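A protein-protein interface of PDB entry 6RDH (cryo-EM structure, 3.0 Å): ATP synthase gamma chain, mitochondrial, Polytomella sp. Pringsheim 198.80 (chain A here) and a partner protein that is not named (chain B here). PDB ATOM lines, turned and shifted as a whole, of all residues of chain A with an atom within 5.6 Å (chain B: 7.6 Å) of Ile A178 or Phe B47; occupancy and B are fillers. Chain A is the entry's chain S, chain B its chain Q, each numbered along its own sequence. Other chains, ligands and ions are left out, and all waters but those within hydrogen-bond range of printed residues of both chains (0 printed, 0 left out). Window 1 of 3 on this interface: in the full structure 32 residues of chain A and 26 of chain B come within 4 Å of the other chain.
Printed residues of chain B within 4 Å of Thr A165: His B46 (3.7 Å) and Phe B47 (3.9 Å).
Of the printed residues of chain B, Gln A174 touches Ile B45 (3.8 Å), His B46 (2.9 Å) and Phe B47 (3.8 Å).
Of the printed residues of chain B, Val A179 touches Leu B17 (3.7 Å).
Printed residues of chain B within 4 Å of Glu A181: Gln B49.
Met A259 touches none of the printed residues of chain B.
Of the printed residues of chain A, His B46 touches Asp A164 (3.2 Å), Thr A165 (3.7 Å) and Gln A174 (2.9 Å).
Of the printed residues of chain A, Phe B47 touches Ile A162, Ala A163, Asp A164, Thr A165, Gln A174, Leu A177 and Ile A178.
The nearest residue of chain B that does not touch Ile A178 is Gln B49 (6.6 Å).
The nearest printed residue of chain A that does not touch His B46 is Ala A163 (5.5 Å).
Phe B47 touches Asp A164 (CA to O, 3.8 Å).
Thr A165 touches His B46 (O to O, 3.7 Å).
Thr A165 touches Phe B47.
Ile B45 touches Gln A174 (CG1 to N, 3.8 Å).
Leu B17 touches Ser A176 (CD1 to O, 3.9 Å).
CD1 of Leu A177 touches CD1 of Ile B45, 3.8 Å away.
Tyr B63 touches Leu A177.
Ile A178 touches Phe B47.
CD1 of Leu B17 touches CB of Val A179, at 3.7 Å.
Glu A181 touches Gln B49 (CG to OE1, 3.3 Å).
Hydrophobic or aromatic side chains of chain B that line the printed part of chain A: Leu B17, Ile B45, Phe B47 and Tyr B63.
Of the 18 printed residues of chain A, 11 touch a printed residue of chain B.
The backbone NH of Ile B45 is in hydrogen-bond range of the backbone carbonyl oxygen of Leu B65 (2.6 Å).
The backbone carbonyl oxygen (O) of Phe B47 lies within hydrogen-bond range of the backbone NH (N) of Tyr B63 (3.1 Å).
The backbone NH (N) of Gln B49 lies within hydrogen-bond range of the backbone carbonyl oxygen (O) of Lys B61.
The side-chain amino group (NZ) of Lys B61 lies within hydrogen-bond range of the side-chain hydroxyl (OH) of Tyr B63 (2.9 Å).
The side-chain amide oxygen of Gln A174 lies within hydrogen-bond range of the side-chain hydroxyl of Thr A165 (2.6 Å).
OG1 of Thr A165 is in hydrogen-bond range of SD of Met A259, 3.5 Å away.
The side-chain amide nitrogen (NE2) of Gln A174 sits at hydrogen-bond distance from the backbone carbonyl oxygen (O) of His B46, at 2.9 Å.
O of Arg B48 lies within hydrogen-bond range of N of Ala A163.
OD1 of Asp A164 is in salt-bridge range of NH2 of Arg B48 (2.9 Å).
The backbone carbonyl oxygen of His B46 sits close to the backbone carbonyl oxygen of Asp A164, at 3.2 Å.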
ATOM      1  N   ILE A 142      -0.554   2.787 -12.592  1.00  0.00           N
ATOM      2  CA  ILE A 142       0.779   2.800 -12.011  1.00  0.00           C
ATOM      3  C   ILE A 142       1.538   3.946 -12.662  1.00  0.00           C
ATOM      4  O   ILE A 142       1.852   3.896 -13.855  1.00  0.00           O
ATOM      5  CB  ILE A 142       1.500   1.461 -12.197  1.00  0.00           C
ATOM      6  CG1 ILE A 142       0.780   0.379 -11.400  1.00  0.00           C
ATOM      7  CG2 ILE A 142       2.929   1.574 -11.743  1.00  0.00           C
ATOM      8  CD1 ILE A 142       1.441  -0.953 -11.446  1.00  0.00           C
ATOM      9  N   ILE A 162      -1.252   4.127  -7.950  1.00  0.00           N
ATOM     10  CA  ILE A 162       0.127   3.901  -7.534  1.00  0.00           C
ATOM     11  C   ILE A 162       1.013   4.874  -8.292  1.00  0.00           C
ATOM     12  O   ILE A 162       0.899   5.007  -9.514  1.00  0.00           O
ATOM     13  CB  ILE A 162       0.562   2.445  -7.783  1.00  0.00           C
ATOM     14  CG1 ILE A 162      -0.203   1.473  -6.896  1.00  0.00           C
ATOM     15  CG2 ILE A 162       2.028   2.258  -7.515  1.00  0.00           C
ATOM     16  CD1 ILE A 162      -1.334   0.791  -7.572  1.00  0.00           C
ATOM     17  N   ALA A 163       1.887   5.568  -7.570  1.00  0.00           N
ATOM     18  CA  ALA A 163       2.802   6.513  -8.172  1.00  0.00           C
ATOM     19  C   ALA A 163       4.146   6.401  -7.472  1.00  0.00           C
ATOM     20  O   ALA A 163       4.320   5.598  -6.556  1.00  0.00           O
ATOM     21  CB  ALA A 163       2.242   7.931  -8.091  1.00  0.00           C
ATOM     22  N   ASP A 164       5.100   7.214  -7.935  1.00  0.00           N
ATOM     23  CA  ASP A 164       6.466   7.323  -7.419  1.00  0.00           C
ATOM     24  C   ASP A 164       7.238   6.012  -7.476  1.00  0.00           C
ATOM     25  O   ASP A 164       8.199   5.829  -6.727  1.00  0.00           O
ATOM     26  CB  ASP A 164       6.491   7.876  -5.987  1.00  0.00           C
ATOM     27  CG  ASP A 164       6.404   9.389  -5.942  1.00  0.00           C
ATOM     28  OD1 ASP A 164       6.015   9.932  -4.886  1.00  0.00           O
ATOM     29  OD2 ASP A 164       6.722  10.036  -6.962  1.00  0.00           O
ATOM     30  N   THR A 165       6.866   5.102  -8.370  1.00  0.00           N
ATOM     31  CA  THR A 165       7.426   3.759  -8.331  1.00  0.00           C
ATOM     32  C   THR A 165       8.788   3.649  -8.993  1.00  0.00           C
ATOM     33  O   THR A 165       9.609   2.840  -8.555  1.00  0.00           O
ATOM     34  CB  THR A 165       6.461   2.764  -8.972  1.00  0.00           C
ATOM     35  OG1 THR A 165       7.151   1.540  -9.232  1.00  0.00           O
ATOM     36  CG2 THR A 165       5.891   3.310 -10.249  1.00  0.00           C
ATOM     37  N   GLY A 173       9.805  -6.781  -4.607  1.00  0.00           N
ATOM     38  CA  GLY A 173       9.005  -6.547  -3.418  1.00  0.00           C
ATOM     39  C   GLY A 173       8.013  -5.421  -3.605  1.00  0.00           C
ATOM     40  O   GLY A 173       6.903  -5.465  -3.068  1.00  0.00           O
ATOM     41  N   GLN A 174       8.382  -4.430  -4.406  1.00  0.00           N
ATOM     42  CA  GLN A 174       7.492  -3.325  -4.725  1.00  0.00           C
ATOM     43  C   GLN A 174       6.324  -3.791  -5.583  1.00  0.00           C
ATOM     44  O   GLN A 174       5.163  -3.468  -5.301  1.00  0.00           O
ATOM     45  CB  GLN A 174       8.303  -2.250  -5.430  1.00  0.00           C
ATOM     46  CG  GLN A 174       7.553  -1.079  -5.928  1.00  0.00           C
ATOM     47  CD  GLN A 174       8.466  -0.186  -6.695  1.00  0.00           C
ATOM     48  OE1 GLN A 174       8.475  -0.200  -7.919  1.00  0.00           O
ATOM     49  NE2 GLN A 174       9.279   0.573  -5.984  1.00  0.00           N
ATOM     50  N   ALA A 175       6.615  -4.572  -6.626  1.00  0.00           N
ATOM     51  CA  ALA A 175       5.561  -5.147  -7.449  1.00  0.00           C
ATOM     52  C   ALA A 175       4.707  -6.126  -6.662  1.00  0.00           C
ATOM     53  O   ALA A 175       3.506  -6.235  -6.912  1.00  0.00           O
ATOM     54  CB  ALA A 175       6.167  -5.837  -8.662  1.00  0.00           C
ATOM     55  N   SER A 176       5.300  -6.804  -5.683  1.00  0.00           N
ATOM     56  CA  SER A 176       4.556  -7.712  -4.825  1.00  0.00           C
ATOM     57  C   SER A 176       3.592  -6.961  -3.923  1.00  0.00           C
ATOM     58  O   SER A 176       2.463  -7.413  -3.716  1.00  0.00           O
ATOM     59  CB  SER A 176       5.524  -8.538  -3.993  1.00  0.00           C
ATOM     60  OG  SER A 176       6.553  -9.051  -4.805  1.00  0.00           O
ATOM     61  N   LEU A 177       4.010  -5.815  -3.382  1.00  0.00           N
ATOM     62  CA  LEU A 177       3.101  -5.019  -2.560  1.00  0.00           C
ATOM     63  C   LEU A 177       1.977  -4.421  -3.393  1.00  0.00           C
ATOM     64  O   LEU A 177       0.828  -4.346  -2.934  1.00  0.00           O
ATOM     65  CB  LEU A 177       3.867  -3.913  -1.848  1.00  0.00           C
ATOM     66  CG  LEU A 177       4.733  -4.276  -0.650  1.00  0.00           C
ATOM     67  CD1 LEU A 177       5.157  -3.019   0.058  1.00  0.00           C
ATOM     68  CD2 LEU A 177       3.985  -5.179   0.295  1.00  0.00           C
ATOM     69  N   ILE A 178       2.283  -4.004  -4.623  1.00  0.00           N
ATOM     70  CA  ILE A 178       1.238  -3.502  -5.512  1.00  0.00           C
ATOM     71  C   ILE A 178       0.262  -4.614  -5.872  1.00  0.00           C
ATOM     72  O   ILE A 178      -0.956  -4.404  -5.906  1.00  0.00           O
ATOM     73  CB  ILE A 178       1.869  -2.866  -6.762  1.00  0.00           C
ATOM     74  CG1 ILE A 178       2.697  -1.656  -6.369  1.00  0.00           C
ATOM     75  CG2 ILE A 178       0.818  -2.404  -7.728  1.00  0.00           C
ATOM     76  CD1 ILE A 178       3.620  -1.204  -7.447  1.00  0.00           C
ATOM     77  N   VAL A 179       0.771  -5.827  -6.083  1.00  0.00           N
ATOM     78  CA  VAL A 179      -0.107  -6.953  -6.363  1.00  0.00           C
ATOM     79  C   VAL A 179      -0.931  -7.339  -5.147  1.00  0.00           C
ATOM     80  O   VAL A 179      -2.078  -7.758  -5.301  1.00  0.00           O
ATOM     81  CB  VAL A 179       0.704  -8.140  -6.857  1.00  0.00           C
ATOM     82  N   GLU A 180      -0.380  -7.188  -3.942  1.00  0.00           N
ATOM     83  CA  GLU A 180      -1.155  -7.419  -2.725  1.00  0.00           C
ATOM     84  C   GLU A 180      -2.309  -6.439  -2.624  1.00  0.00           C
ATOM     85  O   GLU A 180      -3.431  -6.815  -2.264  1.00  0.00           O
ATOM     86  CB  GLU A 180      -0.265  -7.287  -1.499  1.00  0.00           C
ATOM     87  CG  GLU A 180       0.603  -8.476  -1.217  1.00  0.00           C
ATOM     88  CD  GLU A 180       1.264  -8.370   0.132  1.00  0.00           C
ATOM     89  OE1 GLU A 180       0.547  -8.177   1.135  1.00  0.00           O
ATOM     90  OE2 GLU A 180       2.505  -8.442   0.189  1.00  0.00           O
ATOM     91  N   GLU A 181      -2.052  -5.175  -2.956  1.00  0.00           N
ATOM     92  CA  GLU A 181      -3.121  -4.188  -2.962  1.00  0.00           C
ATOM     93  C   GLU A 181      -4.132  -4.428  -4.076  1.00  0.00           C
ATOM     94  O   GLU A 181      -5.287  -4.023  -3.943  1.00  0.00           O
ATOM     95  CB  GLU A 181      -2.535  -2.784  -3.063  1.00  0.00           C
ATOM     96  CG  GLU A 181      -3.473  -1.712  -2.557  1.00  0.00           C
ATOM     97  CD  GLU A 181      -3.776  -1.837  -1.073  1.00  0.00           C
ATOM     98  OE1 GLU A 181      -4.913  -1.511  -0.670  1.00  0.00           O
ATOM     99  OE2 GLU A 181      -2.874  -2.240  -0.307  1.00  0.00           O
ATOM    100  N   LEU A 182      -3.738  -5.083  -5.163  1.00  0.00           N
ATOM    101  CA  LEU A 182      -4.746  -5.473  -6.145  1.00  0.00           C
ATOM    102  C   LEU A 182      -5.544  -6.686  -5.690  1.00  0.00           C
ATOM    103  O   LEU A 182      -6.706  -6.834  -6.074  1.00  0.00           O
ATOM    104  CB  LEU A 182      -4.101  -5.772  -7.494  1.00  0.00           C
ATOM    105  CG  LEU A 182      -3.347  -4.620  -8.148  1.00  0.00           C
ATOM    106  CD1 LEU A 182      -2.859  -5.037  -9.507  1.00  0.00           C
ATOM    107  CD2 LEU A 182      -4.217  -3.401  -8.236  1.00  0.00           C
ATOM    108  N   ILE A 183      -4.933  -7.566  -4.893  1.00  0.00           N
ATOM    109  CA  ILE A 183      -5.612  -8.750  -4.362  1.00  0.00           C
ATOM    110  C   ILE A 183      -6.452  -8.412  -3.132  1.00  0.00           C
ATOM    111  O   ILE A 183      -7.278  -9.232  -2.703  1.00  0.00           O
ATOM    112  CB  ILE A 183      -4.491  -9.807  -4.231  1.00  0.00           C
ATOM    113  CG1 ILE A 183      -4.074 -10.263  -5.620  1.00  0.00           C
ATOM    114  CG2 ILE A 183      -4.882 -11.070  -3.487  1.00  0.00           C
ATOM    115  CD1 ILE A 183      -2.771 -10.980  -5.643  1.00  0.00           C
ATOM    116  N   LEU A 255       3.513  -7.924 -13.237  1.00  0.00           N
ATOM    117  CA  LEU A 255       3.538  -6.520 -12.864  1.00  0.00           C
ATOM    118  C   LEU A 255       4.956  -5.971 -12.836  1.00  0.00           C
ATOM    119  O   LEU A 255       5.201  -4.855 -13.306  1.00  0.00           O
ATOM    120  CB  LEU A 255       2.871  -6.382 -11.508  1.00  0.00           C
ATOM    121  CG  LEU A 255       2.263  -5.072 -11.094  1.00  0.00           C
ATOM    122  CD1 LEU A 255       1.272  -4.668 -12.138  1.00  0.00           C
ATOM    123  CD2 LEU A 255       1.565  -5.352  -9.809  1.00  0.00           C
ATOM    124  N   MET A 259       6.140  -3.019 -15.467  1.00  0.00           N
ATOM    125  CA  MET A 259       6.687  -1.713 -15.164  1.00  0.00           C
ATOM    126  C   MET A 259       8.203  -1.657 -15.286  1.00  0.00           C
ATOM    127  O   MET A 259       8.783  -0.611 -15.009  1.00  0.00           O
ATOM    128  CB  MET A 259       6.226  -1.255 -13.785  1.00  0.00           C
ATOM    129  CG  MET A 259       6.808  -1.980 -12.655  1.00  0.00           C
ATOM    130  SD  MET A 259       6.239  -1.254 -11.127  1.00  0.00           S
ATOM    131  CE  MET A 259       4.862  -2.317 -10.800  1.00  0.00           C
ATOM    132  N   LEU B  17       2.946 -14.008  -2.020  1.00  0.00           N
ATOM    133  CA  LEU B  17       3.960 -13.046  -2.435  1.00  0.00           C
ATOM    134  C   LEU B  17       4.716 -12.489  -1.245  1.00  0.00           C
ATOM    135  O   LEU B  17       5.945 -12.390  -1.280  1.00  0.00           O
ATOM    136  CB  LEU B  17       3.313 -11.908  -3.205  1.00  0.00           C
ATOM    137  CG  LEU B  17       2.951 -12.198  -4.643  1.00  0.00           C
ATOM    138  CD1 LEU B  17       2.092 -11.079  -5.090  1.00  0.00           C
ATOM    139  CD2 LEU B  17       4.207 -12.263  -5.461  1.00  0.00           C
ATOM    140  N   ALA B  44      14.864  -2.897  -1.644  1.00  0.00           N
ATOM    141  CA  ALA B  44      14.198  -1.678  -1.215  1.00  0.00           C
ATOM    142  C   ALA B  44      12.860  -1.502  -1.915  1.00  0.00           C
ATOM    143  O   ALA B  44      12.698  -1.833  -3.088  1.00  0.00           O
ATOM    144  CB  ALA B  44      15.079  -0.463  -1.483  1.00  0.00           C
ATOM    145  N   ILE B  45      11.900  -0.961  -1.178  1.00  0.00           N
ATOM    146  CA  ILE B  45      10.556  -0.718  -1.682  1.00  0.00           C
ATOM    147  C   ILE B  45      10.281   0.768  -1.562  1.00  0.00           C
ATOM    148  O   ILE B  45      10.249   1.307  -0.451  1.00  0.00           O
ATOM    149  CB  ILE B  45       9.503  -1.527  -0.916  1.00  0.00           C
ATOM    150  CG1 ILE B  45       9.752  -3.020  -1.100  1.00  0.00           C
ATOM    151  CG2 ILE B  45       8.117  -1.158  -1.389  1.00  0.00           C
ATOM    152  CD1 ILE B  45       8.815  -3.872  -0.316  1.00  0.00           C
ATOM    153  N   HIS B  46      10.080   1.428  -2.697  1.00  0.00           N
ATOM    154  CA  HIS B  46       9.901   2.879  -2.736  1.00  0.00           C
ATOM    155  C   HIS B  46       8.787   3.195  -3.728  1.00  0.00           C
ATOM    156  O   HIS B  46       9.030   3.274  -4.934  1.00  0.00           O
ATOM    157  CB  HIS B  46      11.194   3.579  -3.122  1.00  0.00           C
ATOM    158  CG  HIS B  46      12.228   3.592  -2.043  1.00  0.00           C
ATOM    159  ND1 HIS B  46      13.466   3.004  -2.192  1.00  0.00           N
ATOM    160  CD2 HIS B  46      12.218   4.139  -0.807  1.00  0.00           C
ATOM    161  CE1 HIS B  46      14.170   3.182  -1.090  1.00  0.00           C
ATOM    162  NE2 HIS B  46      13.437   3.867  -0.234  1.00  0.00           N
ATOM    163  N   PHE B  47       7.579   3.388  -3.215  1.00  0.00           N
ATOM    164  CA  PHE B  47       6.465   3.867  -4.022  1.00  0.00           C
ATOM    165  C   PHE B  47       5.461   4.528  -3.091  1.00  0.00           C
ATOM    166  O   PHE B  47       5.746   4.764  -1.915  1.00  0.00           O
ATOM    167  CB  PHE B  47       5.850   2.740  -4.867  1.00  0.00           C
ATOM    168  CG  PHE B  47       5.005   1.764  -4.098  1.00  0.00           C
ATOM    169  CD1 PHE B  47       5.583   0.836  -3.249  1.00  0.00           C
ATOM    170  CD2 PHE B  47       3.634   1.736  -4.275  1.00  0.00           C
ATOM    171  CE1 PHE B  47       4.808  -0.067  -2.566  1.00  0.00           C
ATOM    172  CE2 PHE B  47       2.855   0.832  -3.595  1.00  0.00           C
ATOM    173  CZ  PHE B  47       3.443  -0.070  -2.743  1.00  0.00           C
ATOM    174  N   ARG B  48       4.298   4.869  -3.632  1.00  0.00           N
ATOM    175  CA  ARG B  48       3.220   5.439  -2.845  1.00  0.00           C
ATOM    176  C   ARG B  48       1.905   5.091  -3.521  1.00  0.00           C
ATOM    177  O   ARG B  48       1.865   4.772  -4.711  1.00  0.00           O
ATOM    178  CB  ARG B  48       3.378   6.955  -2.690  1.00  0.00           C
ATOM    179  CG  ARG B  48       2.902   7.754  -3.875  1.00  0.00           C
ATOM    180  CD  ARG B  48       2.788   9.217  -3.541  1.00  0.00           C
ATOM    181  NE  ARG B  48       1.809   9.867  -4.398  1.00  0.00           N
ATOM    182  CZ  ARG B  48       2.103  10.433  -5.559  1.00  0.00           C
ATOM    183  NH1 ARG B  48       1.149  10.996  -6.284  1.00  0.00           N
ATOM    184  NH2 ARG B  48       3.350  10.430  -5.997  1.00  0.00           N
ATOM    185  N   GLN B  49       0.822   5.139  -2.753  1.00  0.00           N
ATOM    186  CA  GLN B  49      -0.462   4.727  -3.297  1.00  0.00           C
ATOM    187  C   GLN B  49      -1.588   5.484  -2.619  1.00  0.00           C
ATOM    188  O   GLN B  49      -1.445   5.996  -1.507  1.00  0.00           O
ATOM    189  CB  GLN B  49      -0.680   3.224  -3.151  1.00  0.00           C
ATOM    190  CG  GLN B  49      -0.367   2.689  -1.782  1.00  0.00           C
ATOM    191  CD  GLN B  49      -1.159   1.452  -1.478  1.00  0.00           C
ATOM    192  OE1 GLN B  49      -2.258   1.272  -1.991  1.00  0.00           O
ATOM    193  NE2 GLN B  49      -0.611   0.589  -0.639  1.00  0.00           N
ATOM    194  N   ALA B  50      -2.722   5.532  -3.306  1.00  0.00           N
ATOM    195  CA  ALA B  50      -3.851   6.350  -2.899  1.00  0.00           C
ATOM    196  C   ALA B  50      -5.137   5.832  -3.526  1.00  0.00           C
ATOM    197  O   ALA B  50      -5.221   5.724  -4.754  1.00  0.00           O
ATOM    198  CB  ALA B  50      -3.615   7.801  -3.310  1.00  0.00           C
ATOM    199  N   LYS B  61      -0.873   6.860   1.060  1.00  0.00           N
ATOM    200  CA  LYS B  61      -0.094   5.825   1.727  1.00  0.00           C
ATOM    201  C   LYS B  61       1.255   5.779   1.033  1.00  0.00           C
ATOM    202  O   LYS B  61       1.309   5.809  -0.198  1.00  0.00           O
ATOM    203  CB  LYS B  61      -0.805   4.469   1.652  1.00  0.00           C
ATOM    204  CG  LYS B  61      -0.003   3.299   2.180  1.00  0.00           C
ATOM    205  CD  LYS B  61       0.400   3.513   3.623  1.00  0.00           C
ATOM    206  CE  LYS B  61       1.290   2.396   4.121  1.00  0.00           C
ATOM    207  NZ  LYS B  61       0.577   1.099   4.117  1.00  0.00           N
ATOM    208  N   VAL B  62       2.335   5.723   1.806  1.00  0.00           N
ATOM    209  CA  VAL B  62       3.680   5.811   1.253  1.00  0.00           C
ATOM    210  C   VAL B  62       4.532   4.701   1.860  1.00  0.00           C
ATOM    211  O   VAL B  62       4.283   4.255   2.984  1.00  0.00           O
ATOM    212  CB  VAL B  62       4.285   7.218   1.491  1.00  0.00           C
ATOM    213  CG1 VAL B  62       4.565   7.486   2.967  1.00  0.00           C
ATOM    214  CG2 VAL B  62       5.518   7.471   0.626  1.00  0.00           C
ATOM    215  N   TYR B  63       5.502   4.219   1.086  1.00  0.00           N
ATOM    216  CA  TYR B  63       6.405   3.151   1.488  1.00  0.00           C
ATOM    217  C   TYR B  63       7.824   3.592   1.175  1.00  0.00           C
ATOM    218  O   TYR B  63       8.159   3.815   0.010  1.00  0.00           O
ATOM    219  CB  TYR B  63       6.098   1.853   0.744  1.00  0.00           C
ATOM    220  CG  TYR B  63       4.745   1.254   1.014  1.00  0.00           C
ATOM    221  CD1 TYR B  63       3.635   1.657   0.296  1.00  0.00           C
ATOM    222  CD2 TYR B  63       4.585   0.261   1.965  1.00  0.00           C
ATOM    223  CE1 TYR B  63       2.400   1.104   0.527  1.00  0.00           C
ATOM    224  CE2 TYR B  63       3.351  -0.301   2.206  1.00  0.00           C
ATOM    225  CZ  TYR B  63       2.263   0.125   1.484  1.00  0.00           C
ATOM    226  OH  TYR B  63       1.031  -0.434   1.723  1.00  0.00           O
ATOM    227  N   GLU B  64       8.654   3.714   2.204  1.00  0.00           N
ATOM    228  CA  GLU B  64      10.045   4.082   1.983  1.00  0.00           C
ATOM    229  C   GLU B  64      10.943   3.074   2.673  1.00  0.00           C
ATOM    230  O   GLU B  64      11.874   3.430   3.401  1.00  0.00           O
ATOM    231  CB  GLU B  64      10.326   5.505   2.460  1.00  0.00           C
ATOM    232  CG  GLU B  64       9.675   6.560   1.581  1.00  0.00           C
ATOM    233  CD  GLU B  64      10.008   7.967   2.001  1.00  0.00           C
ATOM    234  OE1 GLU B  64      10.638   8.139   3.065  1.00  0.00           O
ATOM    235  OE2 GLU B  64       9.644   8.901   1.256  1.00  0.00           O
ATOM    236  N   LEU B  65      10.646   1.805   2.443  1.00  0.00           N
ATOM    237  CA  LEU B  65      11.336   0.701   3.081  1.00  0.00           C
ATOM    238  C   LEU B  65      12.595   0.387   2.290  1.00  0.00           C
ATOM    239  O   LEU B  65      12.519   0.050   1.106  1.00  0.00           O
ATOM    240  CB  LEU B  65      10.403  -0.503   3.125  1.00  0.00           C
ATOM    241  CG  LEU B  65       9.116  -0.143   3.857  1.00  0.00           C
ATOM    242  CD1 LEU B  65       8.062  -1.203   3.661  1.00  0.00           C
ATOM    243  CD2 LEU B  65       9.404   0.077   5.333  1.00  0.00           C
